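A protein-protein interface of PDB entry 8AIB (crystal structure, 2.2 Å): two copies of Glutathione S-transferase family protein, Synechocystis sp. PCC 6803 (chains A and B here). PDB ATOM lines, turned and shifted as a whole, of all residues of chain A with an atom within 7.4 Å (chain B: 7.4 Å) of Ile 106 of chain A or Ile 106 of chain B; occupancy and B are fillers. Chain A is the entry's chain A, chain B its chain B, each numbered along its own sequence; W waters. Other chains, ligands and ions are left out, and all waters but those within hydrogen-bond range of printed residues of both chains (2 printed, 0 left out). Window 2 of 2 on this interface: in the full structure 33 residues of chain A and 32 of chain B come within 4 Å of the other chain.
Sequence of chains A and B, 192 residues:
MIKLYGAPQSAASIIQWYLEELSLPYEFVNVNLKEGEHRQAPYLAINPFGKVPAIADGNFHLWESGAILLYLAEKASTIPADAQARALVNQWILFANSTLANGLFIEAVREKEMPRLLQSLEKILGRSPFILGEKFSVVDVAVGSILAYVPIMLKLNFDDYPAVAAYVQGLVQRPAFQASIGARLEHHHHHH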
ATOM      1  N   SER A  98     -14.395  31.801  -4.533  1.00  0.00           N
ATOM      2  CA  SER A  98     -13.456  32.445  -3.631  1.00  0.00           C
ATOM      3  C   SER A  98     -14.135  32.903  -2.326  1.00  0.00           C
ATOM      4  O   SER A  98     -14.082  32.169  -1.332  1.00  0.00           O
ATOM      5  CB  SER A  98     -12.691  33.566  -4.342  1.00  0.00           C
ATOM      6  OG  SER A  98     -13.579  34.564  -4.825  1.00  0.00           O
ATOM      7  N   LEU A 100     -17.309  33.069  -1.120  1.00  0.00           N
ATOM      8  CA  LEU A 100     -18.287  32.181  -0.497  1.00  0.00           C
ATOM      9  C   LEU A 100     -17.649  30.900   0.045  1.00  0.00           C
ATOM     10  O   LEU A 100     -17.785  30.628   1.235  1.00  0.00           O
ATOM     11  CB  LEU A 100     -19.437  31.871  -1.460  1.00  0.00           C
ATOM     12  CG  LEU A 100     -20.575  31.027  -0.874  1.00  0.00           C
ATOM     13  CD1 LEU A 100     -21.379  31.829   0.179  1.00  0.00           C
ATOM     14  CD2 LEU A 100     -21.477  30.517  -1.979  1.00  0.00           C
ATOM     15  N   ALA A 101     -16.927  30.147  -0.798  1.00  0.00           N
ATOM     16  CA  ALA A 101     -16.272  28.909  -0.387  1.00  0.00           C
ATOM     17  C   ALA A 101     -15.288  29.121   0.752  1.00  0.00           C
ATOM     18  O   ALA A 101     -15.265  28.313   1.656  1.00  0.00           O
ATOM     19  CB  ALA A 101     -15.580  28.257  -1.575  1.00  0.00           C
ATOM     20  N   ASN A 102     -14.520  30.208   0.754  1.00  0.00           N
ATOM     21  CA  ASN A 102     -13.571  30.492   1.844  1.00  0.00           C
ATOM     22  C   ASN A 102     -14.273  30.865   3.165  1.00  0.00           C
ATOM     23  O   ASN A 102     -13.819  30.457   4.235  1.00  0.00           O
ATOM     24  CB  ASN A 102     -12.603  31.607   1.465  1.00  0.00           C
ATOM     25  CG  ASN A 102     -11.738  31.293   0.270  1.00  0.00           C
ATOM     26  OD1 ASN A 102     -11.625  30.144  -0.165  1.00  0.00           O
ATOM     27  ND2 ASN A 102     -11.131  32.329  -0.323  1.00  0.00           N
ATOM     28  N   GLY A 103     -15.336  31.654   3.084  1.00  0.00           N
ATOM     29  CA  GLY A 103     -16.051  32.087   4.267  1.00  0.00           C
ATOM     30  C   GLY A 103     -16.824  30.978   4.955  1.00  0.00           C
ATOM     31  O   GLY A 103     -17.007  31.011   6.175  1.00  0.00           O
ATOM     32  N   LEU A 104     -17.281  29.990   4.185  1.00  0.00           N
ATOM     33  CA  LEU A 104     -18.030  28.877   4.747  1.00  0.00           C
ATOM     34  C   LEU A 104     -17.107  27.743   5.171  1.00  0.00           C
ATOM     35  O   LEU A 104     -17.324  27.151   6.218  1.00  0.00           O
ATOM     36  CB  LEU A 104     -19.056  28.311   3.743  1.00  0.00           C
ATOM     37  CG  LEU A 104     -20.082  29.267   3.144  1.00  0.00           C
ATOM     38  CD1 LEU A 104     -21.005  28.535   2.176  1.00  0.00           C
ATOM     39  CD2 LEU A 104     -20.891  29.946   4.207  1.00  0.00           C
ATOM     40  N   PHE A 105     -16.096  27.427   4.363  1.00  0.00           N
ATOM     41  CA  PHE A 105     -15.279  26.251   4.579  1.00  0.00           C
ATOM     42  C   PHE A 105     -13.940  26.442   5.304  1.00  0.00           C
ATOM     43  O   PHE A 105     -13.344  25.431   5.656  1.00  0.00           O
ATOM     44  CB  PHE A 105     -15.049  25.537   3.243  1.00  0.00           C
ATOM     45  CG  PHE A 105     -16.326  24.923   2.704  1.00  0.00           C
ATOM     46  CD1 PHE A 105     -16.749  23.676   3.132  1.00  0.00           C
ATOM     47  CD2 PHE A 105     -17.113  25.605   1.795  1.00  0.00           C
ATOM     48  CE1 PHE A 105     -17.925  23.119   2.643  1.00  0.00           C
ATOM     49  CE2 PHE A 105     -18.287  25.054   1.314  1.00  0.00           C
ATOM     50  CZ  PHE A 105     -18.691  23.817   1.742  1.00  0.00           C
ATOM     51  N   ILE A 106     -13.460  27.668   5.534  1.00  0.00           N
ATOM     52  CA  ILE A 106     -12.199  27.859   6.253  1.00  0.00           C
ATOM     53  C   ILE A 106     -12.500  28.189   7.697  1.00  0.00           C
ATOM     54  O   ILE A 106     -13.094  29.218   7.972  1.00  0.00           O
ATOM     55  CB  ILE A 106     -11.289  28.885   5.572  1.00  0.00           C
ATOM     56  CG1 ILE A 106     -10.938  28.412   4.155  1.00  0.00           C
ATOM     57  CG2 ILE A 106     -10.036  29.159   6.419  1.00  0.00           C
ATOM     58  CD1 ILE A 106     -10.305  29.416   3.361  1.00  0.00           C
ATOM     59  N   GLU A 107     -12.144  27.268   8.616  1.00  0.00           N
ATOM     60  CA  GLU A 107     -12.426  27.331  10.056  1.00  0.00           C
ATOM     61  C   GLU A 107     -12.003  28.619  10.753  1.00  0.00           C
ATOM     62  O   GLU A 107     -12.782  29.176  11.540  1.00  0.00           O
ATOM     63  CB  GLU A 107     -11.805  26.123  10.772  1.00  0.00           C
ATOM     64  CG  GLU A 107     -12.215  25.995  12.228  1.00  0.00           C
ATOM     65  CD  GLU A 107     -12.103  24.575  12.745  1.00  0.00           C
ATOM     66  OE1 GLU A 107     -10.960  24.128  13.001  1.00  0.00           O
ATOM     67  OE2 GLU A 107     -13.154  23.906  12.886  1.00  0.00           O
ATOM     68  N   ALA A 108     -10.791  29.105  10.461  1.00  0.00           N
ATOM     69  CA  ALA A 108     -10.284  30.324  11.085  1.00  0.00           C
ATOM     70  C   ALA A 108     -11.087  31.577  10.730  1.00  0.00           C
ATOM     71  O   ALA A 108     -11.008  32.554  11.467  1.00  0.00           O
ATOM     72  CB  ALA A 108      -8.819  30.524  10.743  1.00  0.00           C
ATOM     73  N   VAL A 109     -11.872  31.563   9.635  1.00  0.00           N
ATOM     74  CA  VAL A 109     -12.681  32.736   9.275  1.00  0.00           C
ATOM     75  C   VAL A 109     -14.189  32.476   9.299  1.00  0.00           C
ATOM     76  O   VAL A 109     -14.952  33.428   9.178  1.00  0.00           O
ATOM     77  CB  VAL A 109     -12.262  33.347   7.918  1.00  0.00           C
ATOM     78  CG1 VAL A 109     -10.807  33.796   7.936  1.00  0.00           C
ATOM     79  CG2 VAL A 109     -12.516  32.370   6.780  1.00  0.00           C
ATOM     80  N   ARG A 110     -14.624  31.210   9.435  1.00  0.00           N
ATOM     81  CA  ARG A 110     -16.037  30.840   9.396  1.00  0.00           C
ATOM     82  C   ARG A 110     -16.916  31.570  10.397  1.00  0.00           C
ATOM     83  O   ARG A 110     -18.008  31.989  10.028  1.00  0.00           O
ATOM     84  CB  ARG A 110     -16.227  29.318   9.541  1.00  0.00           C
ATOM     85  CG  ARG A 110     -17.682  28.869   9.387  1.00  0.00           C
ATOM     86  CD  ARG A 110     -17.930  27.432   9.810  1.00  0.00           C
ATOM     87  NE  ARG A 110     -17.221  26.495   8.945  1.00  0.00           N
ATOM     88  CZ  ARG A 110     -16.177  25.765   9.322  1.00  0.00           C
ATOM     89  NH1 ARG A 110     -15.714  25.847  10.564  1.00  0.00           N
ATOM     90  NH2 ARG A 110     -15.581  24.953   8.457  1.00  0.00           N
ATOM     91  N   GLU A 111     -16.460  31.734  11.648  1.00  0.00           N
ATOM     92  CA  GLU A 111     -17.277  32.379  12.676  1.00  0.00           C
ATOM     93  C   GLU A 111     -17.718  33.790  12.309  1.00  0.00           C
ATOM     94  O   GLU A 111     -18.863  34.157  12.562  1.00  0.00           O
ATOM     95  CB  GLU A 111     -16.580  32.355  14.049  1.00  0.00           C
ATOM     96  CG  GLU A 111     -17.472  32.820  15.188  1.00  0.00           C
ATOM     97  CD  GLU A 111     -16.863  32.759  16.576  1.00  0.00           C
ATOM     98  OE1 GLU A 111     -15.962  33.580  16.875  1.00  0.00           O
ATOM     99  OE2 GLU A 111     -17.307  31.900  17.376  1.00  0.00           O
ATOM    100  N   GLU A 113     -17.287  35.191   8.944  1.00  0.00           N
ATOM    101  CA  GLU A 113     -17.733  35.208   7.553  1.00  0.00           C
ATOM    102  C   GLU A 113     -19.093  34.554   7.277  1.00  0.00           C
ATOM    103  O   GLU A 113     -19.921  35.164   6.616  1.00  0.00           O
ATOM    104  CB  GLU A 113     -16.664  34.585   6.637  1.00  0.00           C
ATOM    105  CG  GLU A 113     -15.356  35.349   6.560  1.00  0.00           C
ATOM    106  CD  GLU A 113     -15.508  36.721   5.938  1.00  0.00           C
ATOM    107  OE1 GLU A 113     -15.200  37.719   6.630  1.00  0.00           O
ATOM    108  OE2 GLU A 113     -15.983  36.804   4.779  1.00  0.00           O
ATOM    109  N   LEU A 154     -19.736  19.922   6.350  1.00  0.00           N
ATOM    110  CA  LEU A 154     -19.521  20.564   7.650  1.00  0.00           C
ATOM    111  C   LEU A 154     -20.518  20.124   8.734  1.00  0.00           C
ATOM    112  O   LEU A 154     -20.368  20.521   9.897  1.00  0.00           O
ATOM    113  CB  LEU A 154     -19.610  22.091   7.496  1.00  0.00           C
ATOM    114  CG  LEU A 154     -18.793  22.718   6.372  1.00  0.00           C
ATOM    115  CD1 LEU A 154     -19.108  24.189   6.236  1.00  0.00           C
ATOM    116  CD2 LEU A 154     -17.321  22.501   6.594  1.00  0.00           C
ATOM    117  N   SER B  98      -8.692  31.373  -6.647  1.00  0.00           N
ATOM    118  CA  SER B  98      -9.054  30.204  -5.853  1.00  0.00           C
ATOM    119  C   SER B  98      -7.848  29.272  -5.674  1.00  0.00           C
ATOM    120  O   SER B  98      -7.166  29.395  -4.665  1.00  0.00           O
ATOM    121  CB  SER B  98     -10.276  29.487  -6.438  1.00  0.00           C
ATOM    122  OG  SER B  98      -9.981  29.068  -7.763  1.00  0.00           O
ATOM    123  N   LEU B 100      -4.633  29.139  -6.842  1.00  0.00           N
ATOM    124  CA  LEU B 100      -3.360  29.779  -6.524  1.00  0.00           C
ATOM    125  C   LEU B 100      -3.386  30.492  -5.164  1.00  0.00           C
ATOM    126  O   LEU B 100      -2.567  30.175  -4.309  1.00  0.00           O
ATOM    127  CB  LEU B 100      -2.938  30.721  -7.653  1.00  0.00           C
ATOM    128  CG  LEU B 100      -1.584  31.454  -7.475  1.00  0.00           C
ATOM    129  CD1 LEU B 100      -0.407  30.477  -7.490  1.00  0.00           C
ATOM    130  CD2 LEU B 100      -1.394  32.536  -8.556  1.00  0.00           C
ATOM    131  N   ALA B 101      -4.336  31.411  -4.931  1.00  0.00           N
ATOM    132  CA  ALA B 101      -4.416  32.113  -3.636  1.00  0.00           C
ATOM    133  C   ALA B 101      -4.530  31.154  -2.453  1.00  0.00           C
ATOM    134  O   ALA B 101      -3.840  31.342  -1.459  1.00  0.00           O
ATOM    135  CB  ALA B 101      -5.566  33.089  -3.627  1.00  0.00           C
ATOM    136  N   ASN B 102      -5.371  30.123  -2.556  1.00  0.00           N
ATOM    137  CA  ASN B 102      -5.554  29.150  -1.481  1.00  0.00           C
ATOM    138  C   ASN B 102      -4.297  28.343  -1.206  1.00  0.00           C
ATOM    139  O   ASN B 102      -3.947  28.128  -0.050  1.00  0.00           O
ATOM    140  CB  ASN B 102      -6.697  28.193  -1.824  1.00  0.00           C
ATOM    141  CG  ASN B 102      -8.035  28.882  -1.900  1.00  0.00           C
ATOM    142  OD1 ASN B 102      -8.200  30.034  -1.483  1.00  0.00           O
ATOM    143  ND2 ASN B 102      -9.013  28.192  -2.461  1.00  0.00           N
ATOM    144  N   GLY B 103      -3.648  27.888  -2.268  1.00  0.00           N
ATOM    145  CA  GLY B 103      -2.448  27.082  -2.152  1.00  0.00           C
ATOM    146  C   GLY B 103      -1.265  27.812  -1.570  1.00  0.00           C
ATOM    147  O   GLY B 103      -0.413  27.194  -0.932  1.00  0.00           O
ATOM    148  N   LEU B 104      -1.191  29.126  -1.785  1.00  0.00           N
ATOM    149  CA  LEU B 104      -0.101  29.925  -1.254  1.00  0.00           C
ATOM    150  C   LEU B 104      -0.431  30.487   0.129  1.00  0.00           C
ATOM    151  O   LEU B 104       0.451  30.539   0.976  1.00  0.00           O
ATOM    152  CB  LEU B 104       0.229  31.118  -2.185  1.00  0.00           C
ATOM    153  CG  LEU B 104       0.615  30.833  -3.631  1.00  0.00           C
ATOM    154  CD1 LEU B 104       0.967  32.103  -4.352  1.00  0.00           C
ATOM    155  CD2 LEU B 104       1.755  29.886  -3.727  1.00  0.00           C
ATOM    156  N   PHE B 105      -1.661  30.979   0.342  1.00  0.00           N
ATOM    157  CA  PHE B 105      -1.997  31.703   1.567  1.00  0.00           C
ATOM    158  C   PHE B 105      -2.771  30.937   2.654  1.00  0.00           C
ATOM    159  O   PHE B 105      -2.968  31.516   3.725  1.00  0.00           O
ATOM    160  CB  PHE B 105      -2.739  33.005   1.229  1.00  0.00           C
ATOM    161  CG  PHE B 105      -1.847  33.953   0.457  1.00  0.00           C
ATOM    162  CD1 PHE B 105      -0.988  34.814   1.117  1.00  0.00           C
ATOM    163  CD2 PHE B 105      -1.833  33.948  -0.926  1.00  0.00           C
ATOM    164  CE1 PHE B 105      -0.155  35.666   0.403  1.00  0.00           C
ATOM    165  CE2 PHE B 105      -0.973  34.768  -1.634  1.00  0.00           C
ATOM    166  CZ  PHE B 105      -0.135  35.618  -0.968  1.00  0.00           C
ATOM    167  N   ILE B 106      -3.207  29.686   2.421  1.00  0.00           N
ATOM    168  CA  ILE B 106      -3.875  28.928   3.483  1.00  0.00           C
ATOM    169  C   ILE B 106      -2.814  28.043   4.129  1.00  0.00           C
ATOM    170  O   ILE B 106      -2.242  27.169   3.469  1.00  0.00           O
ATOM    171  CB  ILE B 106      -5.117  28.166   3.006  1.00  0.00           C
ATOM    172  CG1 ILE B 106      -6.182  29.154   2.497  1.00  0.00           C
ATOM    173  CG2 ILE B 106      -5.668  27.272   4.134  1.00  0.00           C
ATOM    174  CD1 ILE B 106      -7.288  28.498   1.802  1.00  0.00           C
ATOM    175  N   GLU B 107      -2.482  28.345   5.396  1.00  0.00           N
ATOM    176  CA  GLU B 107      -1.399  27.705   6.136  1.00  0.00           C
ATOM    177  C   GLU B 107      -1.489  26.189   6.196  1.00  0.00           C
ATOM    178  O   GLU B 107      -0.471  25.519   6.056  1.00  0.00           O
ATOM    179  CB  GLU B 107      -1.268  28.308   7.547  1.00  0.00           C
ATOM    180  CG  GLU B 107       0.105  28.095   8.162  1.00  0.00           C
ATOM    181  CD  GLU B 107       0.418  28.973   9.362  1.00  0.00           C
ATOM    182  OE1 GLU B 107      -0.056  30.134   9.395  1.00  0.00           O
ATOM    183  OE2 GLU B 107       1.151  28.501  10.264  1.00  0.00           O
ATOM    184  N   ALA B 108      -2.688  25.646   6.346  1.00  0.00           N
ATOM    185  CA  ALA B 108      -2.889  24.192   6.408  1.00  0.00           C
ATOM    186  C   ALA B 108      -2.583  23.463   5.099  1.00  0.00           C
ATOM    187  O   ALA B 108      -2.269  22.273   5.140  1.00  0.00           O
ATOM    188  CB  ALA B 108      -4.312  23.876   6.848  1.00  0.00           C
ATOM    189  N   VAL B 109      -2.682  24.144   3.943  1.00  0.00           N
ATOM    190  CA  VAL B 109      -2.415  23.479   2.664  1.00  0.00           C
ATOM    191  C   VAL B 109      -1.135  23.942   1.984  1.00  0.00           C
ATOM    192  O   VAL B 109      -0.715  23.283   1.033  1.00  0.00           O
ATOM    193  CB  VAL B 109      -3.608  23.555   1.686  1.00  0.00           C
ATOM    194  CG1 VAL B 109      -4.864  22.967   2.311  1.00  0.00           C
ATOM    195  CG2 VAL B 109      -3.853  24.981   1.222  1.00  0.00           C
ATOM    196  N   ARG B 110      -0.508  25.043   2.456  1.00  0.00           N
ATOM    197  CA  ARG B 110       0.689  25.641   1.847  1.00  0.00           C
ATOM    198  C   ARG B 110       1.846  24.680   1.624  1.00  0.00           C
ATOM    199  O   ARG B 110       2.386  24.655   0.518  1.00  0.00           O
ATOM    200  CB  ARG B 110       1.181  26.872   2.637  1.00  0.00           C
ATOM    201  CG  ARG B 110       2.402  27.566   2.015  1.00  0.00           C
ATOM    202  CD  ARG B 110       2.966  28.675   2.879  1.00  0.00           C
ATOM    203  NE  ARG B 110       1.961  29.698   3.152  1.00  0.00           N
ATOM    204  CZ  ARG B 110       1.597  30.100   4.365  1.00  0.00           C
ATOM    205  NH1 ARG B 110       2.180  29.592   5.444  1.00  0.00           N
ATOM    206  NH2 ARG B 110       0.656  31.022   4.508  1.00  0.00           N
ATOM    207  N   GLU B 111       2.240  23.885   2.645  1.00  0.00           N
ATOM    208  CA  GLU B 111       3.379  22.961   2.506  1.00  0.00           C
ATOM    209  C   GLU B 111       3.217  22.025   1.334  1.00  0.00           C
ATOM    210  O   GLU B 111       4.173  21.808   0.604  1.00  0.00           O
ATOM    211  CB  GLU B 111       3.653  22.153   3.795  1.00  0.00           C
ATOM    212  CG  GLU B 111       4.223  22.976   4.941  1.00  0.00           C
ATOM    213  CD  GLU B 111       3.947  22.393   6.319  1.00  0.00           C
ATOM    214  OE1 GLU B 111       2.856  21.805   6.514  1.00  0.00           O
ATOM    215  OE2 GLU B 111       4.818  22.538   7.211  1.00  0.00           O
ATOM    216  N   GLU B 113       0.592  22.355  -1.387  1.00  0.00           N
ATOM    217  CA  GLU B 113       0.173  23.082  -2.598  1.00  0.00           C
ATOM    218  C   GLU B 113       1.200  24.017  -3.226  1.00  0.00           C
ATOM    219  O   GLU B 113       1.415  23.942  -4.431  1.00  0.00           O
ATOM    220  CB  GLU B 113      -1.120  23.887  -2.323  1.00  0.00           C
ATOM    221  CG  GLU B 113      -2.355  23.060  -2.051  1.00  0.00           C
ATOM    222  CD  GLU B 113      -2.639  22.137  -3.213  1.00  0.00           C
ATOM    223  OE1 GLU B 113      -2.923  22.655  -4.320  1.00  0.00           O
ATOM    224  OE2 GLU B 113      -2.511  20.903  -3.034  1.00  0.00           O
ATOM    225  N   LEU B 154       4.039  37.035   3.095  1.00  0.00           N
ATOM    226  CA  LEU B 154       4.487  35.765   3.674  1.00  0.00           C
ATOM    227  C   LEU B 154       5.957  35.705   4.054  1.00  0.00           C
ATOM    228  O   LEU B 154       6.385  34.666   4.555  1.00  0.00           O
ATOM    229  CB  LEU B 154       4.214  34.595   2.725  1.00  0.00           C
ATOM    230  CG  LEU B 154       2.785  34.299   2.298  1.00  0.00           C
ATOM    231  CD1 LEU B 154       2.755  33.041   1.448  1.00  0.00           C
ATOM    232  CD2 LEU B 154       1.867  34.135   3.501  1.00  0.00           C
HETATM  233  O   HOH W   1      -9.541  32.230  -2.527  1.00  0.00           O
HETATM  234  O   HOH W   2     -11.621  29.215  -2.774  1.00  0.00           O
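The side-chain amide nitrogen of Asn 102 of chain A lies close to the backbone carbonyl oxygen of Ser 98 of chain A (3.1 Å).
O of Ser 98 of chain B lies close to ND2 of Asn 102 of chain B (3.1 Å).
Among the printed residues, pairs that only touch across the chains: Ile 106 of chain A with Ile 106 of chain B (3.5 Å) and Asn 102 of chain A with Asn 102 of chain B (3.7 Å).
Of the printed residues of chain B, Ile 106 of chain A touches Ile 106 (3.5 Å).
Ile 106 of chain B touches just one residue of chain A: Ile 106.
Of the printed residues of chain A, Asn 102 of chain B touches Asn 102 (3.7 Å).
Of the printed residues of chain B, Asn 102 of chain A touches Asn 102.
Val 109 of chain A touches none of the printed residues of chain B.
Leu 100 of chain A touches none of the printed residues of chain B.
The nearest residue of chain A that does not touch Ile 106 of chain B is Asn 102 of chain A (5.0 Å).
The nearest printed residue of chain A that does not touch Asn 102 of chain B is Ile 106 of chain A (5.3 Å).
Hydrophobic or aromatic side chains of chain A within 4 Å of the printed part of chain B: Ile 106.
Among the printed residues, 2 pairs touch across the chains.
Among the printed residues, no Asp or Glu carboxylate lies within 4 Å of a Lys or Arg side-chain nitrogen of the other chain.
Asn 102 of chain A touches its own counterpart, Asn 102 of chain B.
Ile 106 of chain B touches its own counterpart, Ile 106 of chain A.
Water W1 lies within hydrogen-bond range of the side-chain amide nitrogen (ND2) of Asn 102 of chain A (2.7 Å) and the side-chain amide oxygen (OD1) of Asn 102 of chain B (2.8 Å).
Water W2 lies within hydrogen-bond range of OD1 of Asn 102 of chain A (2.8 Å) and ND2 of Asn 102 of chain B (2.8 Å).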
